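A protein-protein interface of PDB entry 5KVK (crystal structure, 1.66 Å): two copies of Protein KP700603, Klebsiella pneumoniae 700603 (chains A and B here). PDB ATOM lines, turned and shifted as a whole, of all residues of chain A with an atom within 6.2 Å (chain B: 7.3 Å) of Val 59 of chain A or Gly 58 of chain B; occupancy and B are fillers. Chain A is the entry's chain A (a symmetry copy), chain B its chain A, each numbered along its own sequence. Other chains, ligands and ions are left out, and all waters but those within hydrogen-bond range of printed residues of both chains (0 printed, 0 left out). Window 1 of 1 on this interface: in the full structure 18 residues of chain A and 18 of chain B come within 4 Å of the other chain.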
ATOM      1  N   THR A  31      33.859 -19.386 -11.711  1.00  0.00           N
ATOM      2  CA  THR A  31      32.694 -20.220 -11.916  1.00  0.00           C
ATOM      3  C   THR A  31      31.463 -19.310 -11.946  1.00  0.00           C
ATOM      4  O   THR A  31      31.528 -18.161 -11.520  1.00  0.00           O
ATOM      5  CB  THR A  31      32.585 -21.290 -10.788  1.00  0.00           C
ATOM      6  OG1 THR A  31      31.518 -22.220 -11.073  1.00  0.00           O
ATOM      7  CG2 THR A  31      32.395 -20.620  -9.391  1.00  0.00           C
ATOM      8  N   THR A  32      30.329 -19.823 -12.455  1.00  0.00           N
ATOM      9  CA  THR A  32      29.149 -18.984 -12.719  1.00  0.00           C
ATOM     10  C   THR A  32      27.843 -19.707 -12.367  1.00  0.00           C
ATOM     11  O   THR A  32      27.696 -20.924 -12.536  1.00  0.00           O
ATOM     12  CB  THR A  32      29.063 -18.576 -14.238  1.00  0.00           C
ATOM     13  OG1 THR A  32      29.024 -19.760 -15.042  1.00  0.00           O
ATOM     14  CG2 THR A  32      30.292 -17.685 -14.657  1.00  0.00           C
ATOM     15  N   ALA A  33      26.874 -18.925 -11.898  1.00  0.00           N
ATOM     16  CA  ALA A  33      25.506 -19.393 -11.552  1.00  0.00           C
ATOM     17  C   ALA A  33      24.544 -18.381 -12.153  1.00  0.00           C
ATOM     18  O   ALA A  33      24.614 -17.172 -11.856  1.00  0.00           O
ATOM     19  CB  ALA A  33      25.283 -19.479 -10.028  1.00  0.00           C
ATOM     20  N   GLU A  34      23.708 -18.845 -13.083  1.00  0.00           N
ATOM     21  CA  GLU A  34      22.829 -17.998 -13.860  1.00  0.00           C
ATOM     22  C   GLU A  34      21.365 -18.386 -13.712  1.00  0.00           C
ATOM     23  O   GLU A  34      21.042 -19.545 -13.553  1.00  0.00           O
ATOM     24  CB  GLU A  34      23.138 -18.100 -15.358  1.00  0.00           C
ATOM     25  CG  GLU A  34      24.509 -17.506 -15.686  1.00  0.00           C
ATOM     26  CD  GLU A  34      24.826 -17.767 -17.158  1.00  0.00           C
ATOM     27  OE1 GLU A  34      24.214 -17.109 -18.017  1.00  0.00           O
ATOM     28  OE2 GLU A  34      25.654 -18.665 -17.488  1.00  0.00           O
ATOM     29  N   SER A  35      20.506 -17.376 -13.825  1.00  0.00           N
ATOM     30  CA  SER A  35      19.098 -17.683 -13.898  1.00  0.00           C
ATOM     31  C   SER A  35      18.623 -17.091 -15.231  1.00  0.00           C
ATOM     32  O   SER A  35      18.661 -17.792 -16.254  1.00  0.00           O
ATOM     33  CB  SER A  35      18.411 -17.161 -12.632  1.00  0.00           C
ATOM     34  OG  SER A  35      17.094 -17.651 -12.594  1.00  0.00           O
ATOM     35  N   GLY A  39      22.526 -19.332 -19.209  1.00  0.00           N
ATOM     36  CA  GLY A  39      23.678 -20.063 -19.723  1.00  0.00           C
ATOM     37  C   GLY A  39      24.491 -19.238 -20.694  1.00  0.00           C
ATOM     38  O   GLY A  39      25.550 -19.706 -21.152  1.00  0.00           O
ATOM     39  N   ALA A  42      28.064 -18.493 -19.267  1.00  0.00           N
ATOM     40  CA  ALA A  42      28.883 -19.697 -19.449  1.00  0.00           C
ATOM     41  C   ALA A  42      29.270 -19.834 -20.912  1.00  0.00           C
ATOM     42  O   ALA A  42      30.422 -20.163 -21.216  1.00  0.00           O
ATOM     43  CB  ALA A  42      28.146 -20.958 -18.974  1.00  0.00           C
ATOM     44  N   TYR A  55      38.311 -21.674 -16.310  1.00  0.00           N
ATOM     45  CA  TYR A  55      36.876 -21.923 -16.118  1.00  0.00           C
ATOM     46  C   TYR A  55      36.543 -23.345 -16.465  1.00  0.00           C
ATOM     47  O   TYR A  55      36.970 -23.815 -17.507  1.00  0.00           O
ATOM     48  CB  TYR A  55      36.063 -21.010 -17.063  1.00  0.00           C
ATOM     49  CG  TYR A  55      34.561 -21.156 -16.946  1.00  0.00           C
ATOM     50  CD1 TYR A  55      33.837 -20.504 -15.907  1.00  0.00           C
ATOM     51  CD2 TYR A  55      33.857 -21.849 -17.907  1.00  0.00           C
ATOM     52  CE1 TYR A  55      32.458 -20.615 -15.807  1.00  0.00           C
ATOM     53  CE2 TYR A  55      32.487 -21.962 -17.816  1.00  0.00           C
ATOM     54  CZ  TYR A  55      31.808 -21.337 -16.780  1.00  0.00           C
ATOM     55  OH  TYR A  55      30.405 -21.447 -16.739  1.00  0.00           O
ATOM     56  N   THR A  57      33.128 -24.782 -14.785  1.00  0.00           N
ATOM     57  CA  THR A  57      31.843 -25.112 -14.178  1.00  0.00           C
ATOM     58  C   THR A  57      30.894 -23.932 -14.227  1.00  0.00           C
ATOM     59  O   THR A  57      31.185 -22.850 -13.669  1.00  0.00           O
ATOM     60  CB  THR A  57      32.073 -25.542 -12.717  1.00  0.00           C
ATOM     61  OG1 THR A  57      32.883 -26.719 -12.721  1.00  0.00           O
ATOM     62  CG2 THR A  57      30.681 -25.880 -12.085  1.00  0.00           C
ATOM     63  N   GLY A  58      29.717 -24.148 -14.834  1.00  0.00           N
ATOM     64  CA  GLY A  58      28.632 -23.199 -14.704  1.00  0.00           C
ATOM     65  C   GLY A  58      27.330 -23.926 -14.421  1.00  0.00           C
ATOM     66  O   GLY A  58      27.125 -25.081 -14.826  1.00  0.00           O
ATOM     67  N   VAL A  59      26.417 -23.209 -13.735  1.00  0.00           N
ATOM     68  CA  VAL A  59      25.074 -23.776 -13.587  1.00  0.00           C
ATOM     69  C   VAL A  59      24.051 -22.756 -14.047  1.00  0.00           C
ATOM     70  O   VAL A  59      24.253 -21.531 -13.986  1.00  0.00           O
ATOM     71  CB  VAL A  59      24.747 -24.225 -12.145  1.00  0.00           C
ATOM     72  CG1 VAL A  59      25.737 -25.282 -11.744  1.00  0.00           C
ATOM     73  CG2 VAL A  59      24.676 -23.000 -11.142  1.00  0.00           C
ATOM     74  N   VAL A  60      22.907 -23.291 -14.447  1.00  0.00           N
ATOM     75  CA  VAL A  60      21.710 -22.509 -14.763  1.00  0.00           C
ATOM     76  C   VAL A  60      20.613 -23.040 -13.819  1.00  0.00           C
ATOM     77  O   VAL A  60      20.244 -24.216 -13.876  1.00  0.00           O
ATOM     78  CB  VAL A  60      21.313 -22.683 -16.235  1.00  0.00           C
ATOM     79  CG1 VAL A  60      20.047 -21.847 -16.550  1.00  0.00           C
ATOM     80  CG2 VAL A  60      22.464 -22.271 -17.132  1.00  0.00           C
ATOM     81  N   THR A  61      20.078 -22.153 -12.967  1.00  0.00           N
ATOM     82  CA  THR A  61      19.091 -22.531 -11.939  1.00  0.00           C
ATOM     83  C   THR A  61      17.946 -21.544 -12.121  1.00  0.00           C
ATOM     84  O   THR A  61      17.982 -20.442 -11.537  1.00  0.00           O
ATOM     85  CB  THR A  61      19.678 -22.451 -10.525  1.00  0.00           C
ATOM     86  OG1 THR A  61      20.323 -21.160 -10.377  1.00  0.00           O
ATOM     87  CG2 THR A  61      20.717 -23.566 -10.313  1.00  0.00           C
ATOM     88  N   VAL A  70      20.403 -26.907  -6.231  1.00  0.00           N
ATOM     89  CA  VAL A  70      21.775 -26.932  -6.750  1.00  0.00           C
ATOM     90  C   VAL A  70      22.703 -26.066  -5.923  1.00  0.00           C
ATOM     91  O   VAL A  70      23.867 -26.422  -5.720  1.00  0.00           O
ATOM     92  CB  VAL A  70      21.774 -26.514  -8.229  1.00  0.00           C
ATOM     93  CG1 VAL A  70      23.257 -26.395  -8.746  1.00  0.00           C
ATOM     94  CG2 VAL A  70      21.007 -27.576  -8.974  1.00  0.00           C
ATOM     95  N   LEU A  71      22.219 -24.923  -5.447  1.00  0.00           N
ATOM     96  CA  LEU A  71      23.062 -23.910  -4.844  1.00  0.00           C
ATOM     97  C   LEU A  71      22.806 -23.717  -3.354  1.00  0.00           C
ATOM     98  O   LEU A  71      23.466 -22.877  -2.729  1.00  0.00           O
ATOM     99  CB  LEU A  71      22.866 -22.575  -5.565  1.00  0.00           C
ATOM    100  CG  LEU A  71      23.255 -22.637  -7.036  1.00  0.00           C
ATOM    101  CD1 LEU A  71      22.839 -21.375  -7.717  1.00  0.00           C
ATOM    102  CD2 LEU A  71      24.787 -22.811  -7.140  1.00  0.00           C
ATOM    103  N   ILE A  96      27.811 -21.715  -5.624  1.00  0.00           N
ATOM    104  CA  ILE A  96      28.556 -22.218  -6.785  1.00  0.00           C
ATOM    105  C   ILE A  96      30.070 -22.120  -6.530  1.00  0.00           C
ATOM    106  O   ILE A  96      30.833 -22.990  -6.976  1.00  0.00           O
ATOM    107  CB  ILE A  96      28.146 -21.495  -8.087  1.00  0.00           C
ATOM    108  CG1 ILE A  96      28.758 -22.170  -9.362  1.00  0.00           C
ATOM    109  CG2 ILE A  96      28.483 -20.016  -8.023  1.00  0.00           C
ATOM    110  CD1 ILE A  96      28.352 -23.669  -9.505  1.00  0.00           C
ATOM    111  N   LEU A  99      30.657 -25.356  -4.585  1.00  0.00           N
ATOM    112  CA  LEU A  99      30.465 -26.557  -5.404  1.00  0.00           C
ATOM    113  C   LEU A  99      31.623 -26.738  -6.378  1.00  0.00           C
ATOM    114  O   LEU A  99      32.182 -27.835  -6.493  1.00  0.00           O
ATOM    115  CB  LEU A  99      29.154 -26.454  -6.156  1.00  0.00           C
ATOM    116  CG  LEU A  99      28.925 -27.498  -7.229  1.00  0.00           C
ATOM    117  CD1 LEU A  99      29.002 -28.872  -6.617  1.00  0.00           C
ATOM    118  CD2 LEU A  99      27.528 -27.164  -7.825  1.00  0.00           C
ATOM    119  N   LEU B  30      12.579 -31.498 -18.438  1.00  0.00           N
ATOM    120  CA  LEU B  30      13.890 -31.669 -19.059  1.00  0.00           C
ATOM    121  C   LEU B  30      14.991 -31.055 -18.187  1.00  0.00           C
ATOM    122  O   LEU B  30      14.794 -30.056 -17.511  1.00  0.00           O
ATOM    123  CB  LEU B  30      13.910 -30.953 -20.433  1.00  0.00           C
ATOM    124  CG  LEU B  30      15.170 -30.995 -21.262  1.00  0.00           C
ATOM    125  CD1 LEU B  30      15.573 -32.395 -21.705  1.00  0.00           C
ATOM    126  CD2 LEU B  30      14.863 -30.152 -22.531  1.00  0.00           C
ATOM    127  N   THR B  31      16.182 -31.647 -18.235  1.00  0.00           N
ATOM    128  CA  THR B  31      17.373 -31.032 -17.689  1.00  0.00           C
ATOM    129  C   THR B  31      18.529 -31.305 -18.654  1.00  0.00           C
ATOM    130  O   THR B  31      18.432 -32.179 -19.511  1.00  0.00           O
ATOM    131  CB  THR B  31      17.673 -31.595 -16.267  1.00  0.00           C
ATOM    132  OG1 THR B  31      18.764 -30.873 -15.656  1.00  0.00           O
ATOM    133  CG2 THR B  31      17.963 -33.127 -16.315  1.00  0.00           C
ATOM    134  N   THR B  32      19.635 -30.551 -18.521  1.00  0.00           N
ATOM    135  CA  THR B  32      20.721 -30.586 -19.514  1.00  0.00           C
ATOM    136  C   THR B  32      22.103 -30.512 -18.853  1.00  0.00           C
ATOM    137  O   THR B  32      22.313 -29.837 -17.837  1.00  0.00           O
ATOM    138  CB  THR B  32      20.618 -29.379 -20.520  1.00  0.00           C
ATOM    139  OG1 THR B  32      20.652 -28.150 -19.786  1.00  0.00           O
ATOM    140  CG2 THR B  32      19.294 -29.458 -21.368  1.00  0.00           C
ATOM    141  N   ALA B  33      23.061 -31.200 -19.468  1.00  0.00           N
ATOM    142  CA  ALA B  33      24.486 -31.223 -19.047  1.00  0.00           C
ATOM    143  C   ALA B  33      25.309 -31.041 -20.312  1.00  0.00           C
ATOM    144  O   ALA B  33      25.189 -31.823 -21.275  1.00  0.00           O
ATOM    145  CB  ALA B  33      24.874 -32.551 -18.363  1.00  0.00           C
ATOM    146  N   GLU B  34      26.071 -29.948 -20.365  1.00  0.00           N
ATOM    147  CA  GLU B  34      26.804 -29.542 -21.545  1.00  0.00           C
ATOM    148  C   GLU B  34      28.298 -29.414 -21.288  1.00  0.00           C
ATOM    149  O   GLU B  34      28.714 -29.048 -20.208  1.00  0.00           O
ATOM    150  CB  GLU B  34      26.346 -28.165 -22.039  1.00  0.00           C
ATOM    151  CG  GLU B  34      24.911 -28.211 -22.568  1.00  0.00           C
ATOM    152  CD  GLU B  34      24.458 -26.792 -22.906  1.00  0.00           C
ATOM    153  OE1 GLU B  34      24.930 -26.251 -23.921  1.00  0.00           O
ATOM    154  OE2 GLU B  34      23.663 -26.171 -22.142  1.00  0.00           O
ATOM    155  N   ALA B  42      21.072 -24.798 -22.779  1.00  0.00           N
ATOM    156  CA  ALA B  42      20.322 -24.181 -21.678  1.00  0.00           C
ATOM    157  C   ALA B  42      19.792 -22.826 -22.118  1.00  0.00           C
ATOM    158  O   ALA B  42      18.640 -22.491 -21.825  1.00  0.00           O
ATOM    159  CB  ALA B  42      21.188 -24.030 -20.419  1.00  0.00           C
ATOM    160  N   CYS B  46      15.961 -21.467 -22.008  1.00  0.00           N
ATOM    161  CA  CYS B  46      15.518 -20.340 -21.193  1.00  0.00           C
ATOM    162  C   CYS B  46      14.962 -19.215 -22.022  1.00  0.00           C
ATOM    163  O   CYS B  46      14.276 -18.353 -21.453  1.00  0.00           O
ATOM    164  CB  CYS B  46      16.676 -19.821 -20.307  1.00  0.00           C
ATOM    165  SG  CYS B  46      17.257 -21.102 -19.097  1.00  0.00           S
ATOM    166  N   TYR B  55      11.434 -26.825 -17.596  1.00  0.00           N
ATOM    167  CA  TYR B  55      12.895 -26.797 -17.444  1.00  0.00           C
ATOM    168  C   TYR B  55      13.284 -25.862 -16.336  1.00  0.00           C
ATOM    169  O   TYR B  55      12.783 -24.750 -16.296  1.00  0.00           O
ATOM    170  CB  TYR B  55      13.539 -26.272 -18.746  1.00  0.00           C
ATOM    171  CG  TYR B  55      15.052 -26.215 -18.724  1.00  0.00           C
ATOM    172  CD1 TYR B  55      15.836 -27.380 -18.961  1.00  0.00           C
ATOM    173  CD2 TYR B  55      15.695 -25.007 -18.569  1.00  0.00           C
ATOM    174  CE1 TYR B  55      17.222 -27.330 -18.965  1.00  0.00           C
ATOM    175  CE2 TYR B  55      17.072 -24.948 -18.573  1.00  0.00           C
ATOM    176  CZ  TYR B  55      17.813 -26.103 -18.783  1.00  0.00           C
ATOM    177  OH  TYR B  55      19.217 -25.998 -18.815  1.00  0.00           O
ATOM    178  N   ASP B  56      14.271 -26.264 -15.478  1.00  0.00           N
ATOM    179  CA  ASP B  56      14.865 -25.233 -14.625  1.00  0.00           C
ATOM    180  C   ASP B  56      16.328 -25.438 -14.282  1.00  0.00           C
ATOM    181  O   ASP B  56      16.914 -24.530 -13.641  1.00  0.00           O
ATOM    182  CB  ASP B  56      14.096 -25.029 -13.316  1.00  0.00           C
ATOM    183  CG  ASP B  56      14.090 -26.287 -12.385  1.00  0.00           C
ATOM    184  OD1 ASP B  56      14.853 -27.297 -12.599  1.00  0.00           O
ATOM    185  OD2 ASP B  56      13.273 -26.232 -11.466  1.00  0.00           O
ATOM    186  N   THR B  57      16.947 -26.545 -14.703  1.00  0.00           N
ATOM    187  CA  THR B  57      18.309 -26.868 -14.290  1.00  0.00           C
ATOM    188  C   THR B  57      19.166 -27.257 -15.477  1.00  0.00           C
ATOM    189  O   THR B  57      18.863 -28.237 -16.195  1.00  0.00           O
ATOM    190  CB  THR B  57      18.265 -28.024 -13.272  1.00  0.00           C
ATOM    191  OG1 THR B  57      17.540 -27.580 -12.124  1.00  0.00           O
ATOM    192  CG2 THR B  57      19.735 -28.359 -12.852  1.00  0.00           C
ATOM    193  N   GLY B  58      20.283 -26.537 -15.657  1.00  0.00           N
ATOM    194  CA  GLY B  58      21.310 -26.981 -16.577  1.00  0.00           C
ATOM    195  C   GLY B  58      22.680 -26.843 -15.940  1.00  0.00           C
ATOM    196  O   GLY B  58      22.919 -25.976 -15.084  1.00  0.00           O
ATOM    197  N   VAL B  59      23.610 -27.704 -16.401  1.00  0.00           N
ATOM    198  CA  VAL B  59      24.996 -27.507 -15.969  1.00  0.00           C
ATOM    199  C   VAL B  59      25.894 -27.452 -17.190  1.00  0.00           C
ATOM    200  O   VAL B  59      25.617 -28.037 -18.252  1.00  0.00           O
ATOM    201  CB  VAL B  59      25.504 -28.600 -15.002  1.00  0.00           C
ATOM    202  CG1 VAL B  59      24.636 -28.585 -13.775  1.00  0.00           C
ATOM    203  CG2 VAL B  59      25.597 -30.019 -15.703  1.00  0.00           C
ATOM    204  N   VAL B  60      27.023 -26.787 -16.993  1.00  0.00           N
ATOM    205  CA  VAL B  60      28.124 -26.750 -17.956  1.00  0.00           C
ATOM    206  C   VAL B  60      29.348 -27.306 -17.202  1.00  0.00           C
ATOM    207  O   VAL B  60      29.787 -26.734 -16.201  1.00  0.00           O
ATOM    208  CB  VAL B  60      28.374 -25.318 -18.449  1.00  0.00           C
ATOM    209  CG1 VAL B  60      29.540 -25.300 -19.470  1.00  0.00           C
ATOM    210  CG2 VAL B  60      27.109 -24.759 -19.072  1.00  0.00           C
ATOM    211  N   THR B  61      29.909 -28.414 -17.709  1.00  0.00           N
ATOM    212  CA  THR B  61      31.022 -29.118 -17.046  1.00  0.00           C
ATOM    213  C   THR B  61      32.072 -29.291 -18.135  1.00  0.00           C
ATOM    214  O   THR B  61      32.023 -30.286 -18.887  1.00  0.00           O
ATOM    215  CB  THR B  61      30.584 -30.470 -16.472  1.00  0.00           C
ATOM    216  OG1 THR B  61      29.872 -31.192 -17.511  1.00  0.00           O
ATOM    217  CG2 THR B  61      29.651 -30.262 -15.266  1.00  0.00           C
ATOM    218  N   VAL B  70      30.620 -32.526 -10.591  1.00  0.00           N
ATOM    219  CA  VAL B  70      29.206 -32.138 -10.638  1.00  0.00           C
ATOM    220  C   VAL B  70      28.314 -33.314 -10.981  1.00  0.00           C
ATOM    221  O   VAL B  70      27.205 -33.426 -10.452  1.00  0.00           O
ATOM    222  CB  VAL B  70      29.022 -30.977 -11.627  1.00  0.00           C
ATOM    223  CG1 VAL B  70      27.488 -30.660 -11.792  1.00  0.00           C
ATOM    224  CG2 VAL B  70      29.776 -29.804 -11.056  1.00  0.00           C
ATOM    225  N   ILE B  96      22.983 -35.763 -14.253  1.00  0.00           N
ATOM    226  CA  ILE B  96      22.156 -34.551 -14.199  1.00  0.00           C
ATOM    227  C   ILE B  96      20.674 -34.925 -14.022  1.00  0.00           C
ATOM    228  O   ILE B  96      19.929 -34.208 -13.339  1.00  0.00           O
ATOM    229  CB  ILE B  96      22.375 -33.651 -15.434  1.00  0.00           C
ATOM    230  CG1 ILE B  96      21.679 -32.254 -15.286  1.00  0.00           C
ATOM    231  CG2 ILE B  96      21.948 -34.354 -16.710  1.00  0.00           C
ATOM    232  CD1 ILE B  96      22.168 -31.466 -14.033  1.00  0.00           C
ATOM    233  N   LEU B  99      20.516 -35.362 -10.229  1.00  0.00           N
ATOM    234  CA  LEU B  99      20.701 -34.102  -9.502  1.00  0.00           C
ATOM    235  C   LEU B  99      19.462 -33.223  -9.618  1.00  0.00           C
ATOM    236  O   LEU B  99      18.969 -32.694  -8.615  1.00  0.00           O
ATOM    237  CB  LEU B  99      21.915 -33.377 -10.045  1.00  0.00           C
ATOM    238  CG  LEU B  99      22.100 -31.950  -9.568  1.00  0.00           C
ATOM    239  CD1 LEU B  99      22.182 -31.931  -8.064  1.00  0.00           C
ATOM    240  CD2 LEU B  99      23.401 -31.458 -10.264  1.00  0.00           C
ATOM    241  N   ALA B 100      18.915 -33.105 -10.837  1.00  0.00           N
ATOM    242  CA  ALA B 100      17.838 -32.153 -11.128  1.00  0.00           C
ATOM    243  C   ALA B 100      16.459 -32.707 -10.791  1.00  0.00           C
ATOM    244  O   ALA B 100      15.487 -31.947 -10.752  1.00  0.00           O
ATOM    245  CB  ALA B 100      17.899 -31.773 -12.630  1.00  0.00           C
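Among the printed residues, pairs that only touch across the chains: Val 60 of chain A with Thr 57 of chain B, Thr 57 of chain A with Val 60 of chain B, Thr 61 of chain A with Asp 56 of chain B, Gly 58 of chain A with Val 59 of chain B, Val 59 of chain A with Gly 58 of chain B, Val 60 of chain A with Cys 46 of chain B, Val 60 of chain A with Ala 42 of chain B and Ala 42 of chain A with Val 60 of chain B.
The backbone NH (N) of Glu 34 of chain B lies within hydrogen-bond range of the backbone carbonyl oxygen (O) of Val 59 of chain B, 2.9 Å away. O of Thr 57 of chain A is in hydrogen-bond range of N of Thr 32 of chain A, 3.4 Å away. The backbone NH (N) of Gly 58 of chain A lies close to the side-chain hydroxyl (OH) of Tyr 55 of chain A, at 3.4 Å. OE2 of Glu 34 of chain B lies within hydrogen-bond range of N of Ala 42 of chain B (3.0 Å). The side-chain hydroxyl (OG1) of Thr 31 of chain A is in hydrogen-bond range of the backbone carbonyl oxygen (O) of Thr 57 of chain A. The backbone carbonyl oxygen of Val 59 of chain A sits at hydrogen-bond distance from the backbone NH of Glu 34 of chain A.
Ala 42 of chain A touches Val 60 of chain B, and with the chains exchanged Val 60 of chain A touches Ala 42 of chain B. Thr 57 of chain A touches Val 60 of chain B, and with the chains exchanged Val 60 of chain A touches Thr 57 of chain B. Gly 58 of chain A touches Val 59 of chain B, and with the chains exchanged Val 59 of chain A touches Gly 58 of chain B. Gly 58 of chain A touches Val 60 of chain B, and with the chains exchanged Val 60 of chain A touches Gly 58 of chain B.
Val 59 of chain A touches just one residue of chain B: Gly 58. Of chain A, only Val 59 (3.4 Å) and Val 60 (2.8 Å) come within 4 Å of Gly 58 of chain B. Of the printed residues of chain A, Ala 42 of chain B touches Val 60 (3.9 Å). Of the printed residues of chain B, Thr 57 of chain A touches Val 60. Of the printed residues of chain B, Gly 58 of chain A touches Val 59 and Val 60. Printed residues of chain A within 4 Å of Thr 57 of chain B: Val 60. Of the printed residues of chain A, Asp 56 of chain B touches Val 60 and Thr 61. Thr 31 of chain A touches none of the printed residues of chain B. The nearest residue of chain B that does not touch Val 59 of chain A is Val 59 of chain B (4.03 Å).
The backbone carbonyl oxygen (O) of Val 60 of chain A lies close to the backbone carbonyl oxygen (O) of Asp 56 of chain B (3.4 Å). N of Val 60 of chain B sits at hydrogen-bond distance from O of Gly 58 of chain A, 2.8 Å away. The backbone carbonyl oxygen of Gly 58 of chain B sits at hydrogen-bond distance from the backbone NH of Val 60 of chain A (2.8 Å).
Of the 17 printed residues of chain A, 6 touch a printed residue of chain B. Hydrophobic or aromatic side chains of chain B that line the printed part of chain A: Ala 42, Val 59 and Val 60. Among the printed residues, 11 pairs touch across the chains. Among the printed residues, no Asp or Glu carboxylate lies within 4 Å of a Lys or Arg side-chain nitrogen of the other chain.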
